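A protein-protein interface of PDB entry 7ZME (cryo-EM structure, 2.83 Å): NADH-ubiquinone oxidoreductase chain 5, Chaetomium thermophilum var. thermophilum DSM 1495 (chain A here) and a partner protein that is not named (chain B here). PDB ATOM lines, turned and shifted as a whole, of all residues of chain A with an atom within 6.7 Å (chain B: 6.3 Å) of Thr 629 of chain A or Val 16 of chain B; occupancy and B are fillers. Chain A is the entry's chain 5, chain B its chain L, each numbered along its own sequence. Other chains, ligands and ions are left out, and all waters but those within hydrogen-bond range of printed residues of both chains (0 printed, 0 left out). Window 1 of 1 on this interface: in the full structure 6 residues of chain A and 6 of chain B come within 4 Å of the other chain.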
ATOM      1  N   SER A 626     -18.936   2.267  -8.414  1.00  0.00           N
ATOM      2  CA  SER A 626     -18.595   2.241  -6.969  1.00  0.00           C
ATOM      3  C   SER A 626     -19.837   2.489  -6.101  1.00  0.00           C
ATOM      4  O   SER A 626     -19.678   2.943  -4.956  1.00  0.00           O
ATOM      5  CB  SER A 626     -17.459   3.140  -6.626  1.00  0.00           C
ATOM      6  OG  SER A 626     -16.993   2.802  -5.338  1.00  0.00           O
ATOM      7  N   HIS A 627     -21.030   2.205  -6.624  1.00  0.00           N
ATOM      8  CA  HIS A 627     -22.250   2.303  -5.783  1.00  0.00           C
ATOM      9  C   HIS A 627     -22.655   0.886  -5.376  1.00  0.00           C
ATOM     10  O   HIS A 627     -22.912   0.088  -6.278  1.00  0.00           O
ATOM     11  CB  HIS A 627     -23.338   3.148  -6.445  1.00  0.00           C
ATOM     12  CG  HIS A 627     -24.322   3.680  -5.460  1.00  0.00           C
ATOM     13  ND1 HIS A 627     -25.682   3.674  -5.692  1.00  0.00           N
ATOM     14  CD2 HIS A 627     -24.149   4.212  -4.231  1.00  0.00           C
ATOM     15  CE1 HIS A 627     -26.304   4.193  -4.654  1.00  0.00           C
ATOM     16  NE2 HIS A 627     -25.384   4.529  -3.742  1.00  0.00           N
ATOM     17  N   VAL A 628     -22.741   0.613  -4.074  1.00  0.00           N
ATOM     18  CA  VAL A 628     -22.988  -0.759  -3.544  1.00  0.00           C
ATOM     19  C   VAL A 628     -24.353  -1.286  -3.998  1.00  0.00           C
ATOM     20  O   VAL A 628     -24.462  -2.487  -4.242  1.00  0.00           O
ATOM     21  CB  VAL A 628     -22.803  -0.780  -2.014  1.00  0.00           C
ATOM     22  CG1 VAL A 628     -23.680   0.245  -1.311  1.00  0.00           C
ATOM     23  CG2 VAL A 628     -22.987  -2.164  -1.416  1.00  0.00           C
ATOM     24  N   THR A 629     -25.355  -0.416  -4.083  1.00  0.00           N
ATOM     25  CA  THR A 629     -26.686  -0.851  -4.554  1.00  0.00           C
ATOM     26  C   THR A 629     -26.613  -1.345  -6.007  1.00  0.00           C
ATOM     27  O   THR A 629     -27.259  -2.359  -6.308  1.00  0.00           O
ATOM     28  CB  THR A 629     -27.719   0.248  -4.291  1.00  0.00           C
ATOM     29  OG1 THR A 629     -27.480   1.313  -5.208  1.00  0.00           O
ATOM     30  CG2 THR A 629     -27.663   0.761  -2.869  1.00  0.00           C
ATOM     31  N   THR A 630     -25.876  -0.645  -6.868  1.00  0.00           N
ATOM     32  CA  THR A 630     -25.724  -1.065  -8.284  1.00  0.00           C
ATOM     33  C   THR A 630     -24.957  -2.378  -8.318  1.00  0.00           C
ATOM     34  O   THR A 630     -25.319  -3.252  -9.115  1.00  0.00           O
ATOM     35  CB  THR A 630     -25.009  -0.005  -9.134  1.00  0.00           C
ATOM     36  OG1 THR A 630     -25.405   1.288  -8.676  1.00  0.00           O
ATOM     37  CG2 THR A 630     -25.295  -0.129 -10.612  1.00  0.00           C
ATOM     38  N   TYR A 631     -23.973  -2.513  -7.432  1.00  0.00           N
ATOM     39  CA  TYR A 631     -23.103  -3.703  -7.473  1.00  0.00           C
ATOM     40  C   TYR A 631     -23.866  -4.856  -6.834  1.00  0.00           C
ATOM     41  O   TYR A 631     -23.659  -5.995  -7.258  1.00  0.00           O
ATOM     42  CB  TYR A 631     -21.813  -3.377  -6.723  1.00  0.00           C
ATOM     43  CG  TYR A 631     -20.797  -2.557  -7.472  1.00  0.00           C
ATOM     44  CD1 TYR A 631     -21.016  -2.145  -8.775  1.00  0.00           C
ATOM     45  CD2 TYR A 631     -19.603  -2.200  -6.868  1.00  0.00           C
ATOM     46  CE1 TYR A 631     -20.076  -1.393  -9.458  1.00  0.00           C
ATOM     47  CE2 TYR A 631     -18.653  -1.452  -7.537  1.00  0.00           C
ATOM     48  CZ  TYR A 631     -18.890  -1.050  -8.837  1.00  0.00           C
ATOM     49  OH  TYR A 631     -17.958  -0.310  -9.498  1.00  0.00           O
ATOM     50  N   ALA A 632     -24.719  -4.572  -5.853  1.00  0.00           N
ATOM     51  CA  ALA A 632     -25.602  -5.629  -5.312  1.00  0.00           C
ATOM     52  C   ALA A 632     -26.524  -6.119  -6.420  1.00  0.00           C
ATOM     53  O   ALA A 632     -26.712  -7.332  -6.531  1.00  0.00           O
ATOM     54  CB  ALA A 632     -26.401  -5.092  -4.157  1.00  0.00           C
ATOM     55  N   LEU A 633     -27.086  -5.190  -7.192  1.00  0.00           N
ATOM     56  CA  LEU A 633     -27.986  -5.586  -8.267  1.00  0.00           C
ATOM     57  C   LEU A 633     -27.265  -6.396  -9.336  1.00  0.00           C
ATOM     58  O   LEU A 633     -27.833  -7.354  -9.862  1.00  0.00           O
ATOM     59  CB  LEU A 633     -28.650  -4.356  -8.879  1.00  0.00           C
ATOM     60  CG  LEU A 633     -29.661  -4.654  -9.984  1.00  0.00           C
ATOM     61  CD1 LEU A 633     -30.707  -5.642  -9.499  1.00  0.00           C
ATOM     62  CD2 LEU A 633     -30.315  -3.390 -10.480  1.00  0.00           C
ATOM     63  N   TYR A 634     -26.025  -6.032  -9.668  1.00  0.00           N
ATOM     64  CA  TYR A 634     -25.248  -6.852 -10.592  1.00  0.00           C
ATOM     65  C   TYR A 634     -25.094  -8.268 -10.057  1.00  0.00           C
ATOM     66  O   TYR A 634     -25.255  -9.241 -10.802  1.00  0.00           O
ATOM     67  CB  TYR A 634     -23.868  -6.236 -10.830  1.00  0.00           C
ATOM     68  CG  TYR A 634     -23.853  -4.904 -11.541  1.00  0.00           C
ATOM     69  CD1 TYR A 634     -24.982  -4.404 -12.166  1.00  0.00           C
ATOM     70  CD2 TYR A 634     -22.695  -4.145 -11.584  1.00  0.00           C
ATOM     71  CE1 TYR A 634     -24.957  -3.182 -12.809  1.00  0.00           C
ATOM     72  CE2 TYR A 634     -22.660  -2.930 -12.224  1.00  0.00           C
ATOM     73  CZ  TYR A 634     -23.789  -2.454 -12.836  1.00  0.00           C
ATOM     74  OH  TYR A 634     -23.747  -1.237 -13.472  1.00  0.00           O
ATOM     75  N   ILE A 635     -24.786  -8.399  -8.765  1.00  0.00           N
ATOM     76  CA  ILE A 635     -24.627  -9.714  -8.151  1.00  0.00           C
ATOM     77  C   ILE A 635     -25.929 -10.497  -8.220  1.00  0.00           C
ATOM     78  O   ILE A 635     -25.936 -11.692  -8.536  1.00  0.00           O
ATOM     79  CB  ILE A 635     -24.137  -9.568  -6.699  1.00  0.00           C
ATOM     80  CG1 ILE A 635     -22.671  -9.151  -6.670  1.00  0.00           C
ATOM     81  CG2 ILE A 635     -24.322 -10.871  -5.936  1.00  0.00           C
ATOM     82  CD1 ILE A 635     -22.242  -8.588  -5.352  1.00  0.00           C
ATOM     83  N   LEU A 636     -27.051  -9.839  -7.925  1.00  0.00           N
ATOM     84  CA  LEU A 636     -28.344 -10.512  -7.968  1.00  0.00           C
ATOM     85  C   LEU A 636     -28.697 -10.944  -9.386  1.00  0.00           C
ATOM     86  O   LEU A 636     -29.277 -12.015  -9.589  1.00  0.00           O
ATOM     87  CB  LEU A 636     -29.426  -9.598  -7.397  1.00  0.00           C
ATOM     88  CG  LEU A 636     -30.865 -10.112  -7.428  1.00  0.00           C
ATOM     89  CD1 LEU A 636     -30.983 -11.416  -6.667  1.00  0.00           C
ATOM     90  CD2 LEU A 636     -31.795  -9.070  -6.851  1.00  0.00           C
ATOM     91  N   GLY B  11     -35.656  -9.611   2.392  1.00  0.00           N
ATOM     92  CA  GLY B  11     -34.313  -9.172   2.729  1.00  0.00           C
ATOM     93  C   GLY B  11     -33.422  -8.993   1.516  1.00  0.00           C
ATOM     94  O   GLY B  11     -32.565  -8.108   1.492  1.00  0.00           O
ATOM     95  N   ILE B  12     -33.601  -9.834   0.494  1.00  0.00           N
ATOM     96  CA  ILE B  12     -32.757  -9.736  -0.690  1.00  0.00           C
ATOM     97  C   ILE B  12     -33.098  -8.486  -1.497  1.00  0.00           C
ATOM     98  O   ILE B  12     -32.200  -7.801  -1.999  1.00  0.00           O
ATOM     99  CB  ILE B  12     -32.841 -11.030  -1.529  1.00  0.00           C
ATOM    100  CG1 ILE B  12     -31.629 -11.161  -2.451  1.00  0.00           C
ATOM    101  CG2 ILE B  12     -34.102 -11.111  -2.338  1.00  0.00           C
ATOM    102  CD1 ILE B  12     -30.381 -11.583  -1.755  1.00  0.00           C
ATOM    103  N   LEU B  13     -34.387  -8.157  -1.633  1.00  0.00           N
ATOM    104  CA  LEU B  13     -34.742  -6.912  -2.305  1.00  0.00           C
ATOM    105  C   LEU B  13     -34.530  -5.693  -1.418  1.00  0.00           C
ATOM    106  O   LEU B  13     -34.161  -4.629  -1.921  1.00  0.00           O
ATOM    107  CB  LEU B  13     -36.185  -6.940  -2.809  1.00  0.00           C
ATOM    108  CG  LEU B  13     -36.527  -7.704  -4.090  1.00  0.00           C
ATOM    109  CD1 LEU B  13     -36.478  -9.202  -3.953  1.00  0.00           C
ATOM    110  CD2 LEU B  13     -37.883  -7.264  -4.592  1.00  0.00           C
ATOM    111  N   GLY B  14     -34.754  -5.818  -0.112  1.00  0.00           N
ATOM    112  CA  GLY B  14     -34.460  -4.705   0.768  1.00  0.00           C
ATOM    113  C   GLY B  14     -32.993  -4.339   0.823  1.00  0.00           C
ATOM    114  O   GLY B  14     -32.665  -3.227   1.250  1.00  0.00           O
ATOM    115  N   PHE B  15     -32.110  -5.248   0.415  1.00  0.00           N
ATOM    116  CA  PHE B  15     -30.680  -4.997   0.302  1.00  0.00           C
ATOM    117  C   PHE B  15     -30.304  -4.486  -1.081  1.00  0.00           C
ATOM    118  O   PHE B  15     -29.502  -3.558  -1.206  1.00  0.00           O
ATOM    119  CB  PHE B  15     -29.902  -6.282   0.616  1.00  0.00           C
ATOM    120  CG  PHE B  15     -28.414  -6.136   0.504  1.00  0.00           C
ATOM    121  CD1 PHE B  15     -27.673  -5.623   1.557  1.00  0.00           C
ATOM    122  CD2 PHE B  15     -27.752  -6.513  -0.654  1.00  0.00           C
ATOM    123  CE1 PHE B  15     -26.303  -5.486   1.463  1.00  0.00           C
ATOM    124  CE2 PHE B  15     -26.382  -6.375  -0.760  1.00  0.00           C
ATOM    125  CZ  PHE B  15     -25.656  -5.863   0.301  1.00  0.00           C
ATOM    126  N   VAL B  16     -30.885  -5.074  -2.124  1.00  0.00           N
ATOM    127  CA  VAL B  16     -30.511  -4.718  -3.486  1.00  0.00           C
ATOM    128  C   VAL B  16     -31.277  -3.490  -3.957  1.00  0.00           C
ATOM    129  O   VAL B  16     -30.711  -2.598  -4.600  1.00  0.00           O
ATOM    130  CB  VAL B  16     -30.731  -5.918  -4.421  1.00  0.00           C
ATOM    131  CG1 VAL B  16     -30.456  -5.524  -5.836  1.00  0.00           C
ATOM    132  CG2 VAL B  16     -29.816  -7.059  -4.023  1.00  0.00           C
ATOM    133  N   LEU B  17     -32.585  -3.455  -3.712  1.00  0.00           N
ATOM    134  CA  LEU B  17     -33.427  -2.339  -4.223  1.00  0.00           C
ATOM    135  C   LEU B  17     -33.570  -1.286  -3.134  1.00  0.00           C
ATOM    136  O   LEU B  17     -34.615  -0.627  -3.097  1.00  0.00           O
ATOM    137  CB  LEU B  17     -34.803  -2.853  -4.673  1.00  0.00           C
ATOM    138  CG  LEU B  17     -34.856  -3.632  -5.987  1.00  0.00           C
ATOM    139  CD1 LEU B  17     -33.993  -2.977  -7.053  1.00  0.00           C
ATOM    140  CD2 LEU B  17     -34.449  -5.081  -5.785  1.00  0.00           C
ATOM    141  N   ASN B  18     -32.532  -1.112  -2.316  1.00  0.00           N
ATOM    142  CA  ASN B  18     -32.562  -0.082  -1.242  1.00  0.00           C
ATOM    143  C   ASN B  18     -32.061   1.254  -1.789  1.00  0.00           C
ATOM    144  O   ASN B  18     -30.960   1.279  -2.350  1.00  0.00           O
ATOM    145  CB  ASN B  18     -31.725  -0.481  -0.021  1.00  0.00           C
ATOM    146  CG  ASN B  18     -32.055   0.355   1.197  1.00  0.00           C
ATOM    147  OD1 ASN B  18     -33.170   0.851   1.332  1.00  0.00           O
ATOM    148  ND2 ASN B  18     -31.096   0.518   2.087  1.00  0.00           N
ATOM    149  N   ARG B  19     -32.836   2.320  -1.626  1.00  0.00           N
ATOM    150  CA  ARG B  19     -32.410   3.669  -2.072  1.00  0.00           C
ATOM    151  C   ARG B  19     -32.541   4.612  -0.877  1.00  0.00           C
ATOM    152  O   ARG B  19     -32.800   5.809  -1.101  1.00  0.00           O
ATOM    153  CB  ARG B  19     -33.291   4.172  -3.219  1.00  0.00           C
ATOM    154  CG  ARG B  19     -33.015   3.534  -4.574  1.00  0.00           C
ATOM    155  CD  ARG B  19     -33.784   2.244  -4.796  1.00  0.00           C
ATOM    156  NE  ARG B  19     -33.552   1.626  -6.094  1.00  0.00           N
ATOM    157  CZ  ARG B  19     -32.554   0.796  -6.369  1.00  0.00           C
ATOM    158  NH1 ARG B  19     -32.436   0.283  -7.582  1.00  0.00           N
ATOM    159  NH2 ARG B  19     -31.671   0.489  -5.437  1.00  0.00           N
ATOM    160  N   MET B  25     -29.695  -1.354   4.639  1.00  0.00           N
ATOM    161  CA  MET B  25     -29.044  -2.520   3.986  1.00  0.00           C
ATOM    162  C   MET B  25     -28.552  -3.508   5.054  1.00  0.00           C
ATOM    163  O   MET B  25     -28.746  -4.711   4.843  1.00  0.00           O
ATOM    164  CB  MET B  25     -27.884  -2.061   3.096  1.00  0.00           C
ATOM    165  CG  MET B  25     -28.326  -1.270   1.889  1.00  0.00           C
ATOM    166  SD  MET B  25     -26.945  -0.718   0.864  1.00  0.00           S
ATOM    167  CE  MET B  25     -26.629  -2.194  -0.099  1.00  0.00           C
ATOM    168  N   SER B  28     -31.447  -5.560   6.194  1.00  0.00           N
ATOM    169  CA  SER B  28     -31.914  -6.564   5.208  1.00  0.00           C
ATOM    170  C   SER B  28     -31.044  -7.808   5.317  1.00  0.00           C
ATOM    171  O   SER B  28     -31.594  -8.906   5.189  1.00  0.00           O
ATOM    172  CB  SER B  28     -31.918  -5.970   3.851  1.00  0.00           C
ATOM    173  OG  SER B  28     -32.758  -4.831   3.835  1.00  0.00           O
ATOM    174  N   ILE B  86     -27.606   6.340   0.894  1.00  0.00           N
ATOM    175  CA  ILE B  86     -27.256   5.963  -0.494  1.00  0.00           C
ATOM    176  C   ILE B  86     -27.945   6.982  -1.398  1.00  0.00           C
ATOM    177  O   ILE B  86     -29.114   7.313  -1.115  1.00  0.00           O
ATOM    178  CB  ILE B  86     -27.654   4.504  -0.767  1.00  0.00           C
ATOM    179  CG1 ILE B  86     -29.068   4.177  -0.290  1.00  0.00           C
ATOM    180  CG2 ILE B  86     -26.645   3.556  -0.138  1.00  0.00           C
ATOM    181  CD1 ILE B  86     -29.222   2.741   0.155  1.00  0.00           C
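Hydrophobic or aromatic side chains of chain B that line the printed part of chain A: Phe 15, Val 16, Met 25 and Ile 86.
Of the 11 printed residues of chain A, 6 touch a printed residue of chain B.
Printed residues of chain A that touch a printed residue of chain B: His 627, Val 628, Thr 629, Ala 632, Leu 633 and Leu 636.
His 627 of chain A touches Ile 86 of chain B (NE2 to CB, 3.7 Å).
CE of Met 25 of chain B touches CG2 of Val 628 of chain A (3.9 Å).
Thr 629 of chain A touches Val 16 of chain B (O to O, 3.9 Å).
Thr 629 of chain A touches Asn 18 of chain B.
Thr 629 of chain A touches Ile 86 of chain B (CG2 to CD1, 3.9 Å).
Ala 632 of chain A touches Phe 15 of chain B.
Ala 632 of chain A touches Val 16 of chain B (CB to CG2, 3.9 Å).
Val 16 of chain B touches Leu 633 of chain A.
Leu 636 of chain A touches Val 16 of chain B.
Thr 629 of chain A touches just these residues of chain B: Val 16 (3.9 Å), Asn 18 (3.4 Å) and Ile 86 (3.9 Å).
Of the printed residues of chain B, Ala 632 of chain A touches Phe 15 (3.6 Å) and Val 16 (3.9 Å).
Of the printed residues of chain B, Val 628 of chain A touches Met 25.
Of the printed residues of chain B, Leu 633 of chain A touches Val 16 (3.5 Å).
Printed residues of chain A within 4 Å of Asn 18 of chain B: Thr 629 (3.4 Å).
Printed residues of chain A within 4 Å of Phe 15 of chain B: Ala 632 (3.6 Å).
Gly 11 of chain B touches none of the printed residues of chain A.
Tyr 631 of chain A touches none of the printed residues of chain B.
The nearest residue of chain B that does not touch Thr 629 of chain A is Met 25 of chain B (4.1 Å).
The nearest residue of chain A that does not touch Val 16 of chain B is Thr 630 of chain A (5.7 Å).
O of Val 16 of chain B lies within hydrogen-bond range of NH2 of Arg 19 of chain B (3.3 Å).
N of Met 25 of chain B sits close to ND2 of Asn 18 of chain B, 3.5 Å away.
A ring nitrogen (ND1) of His 627 of chain A sits at hydrogen-bond distance from the side-chain hydroxyl (OG1) of Thr 629 of chain A (3.0 Å).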
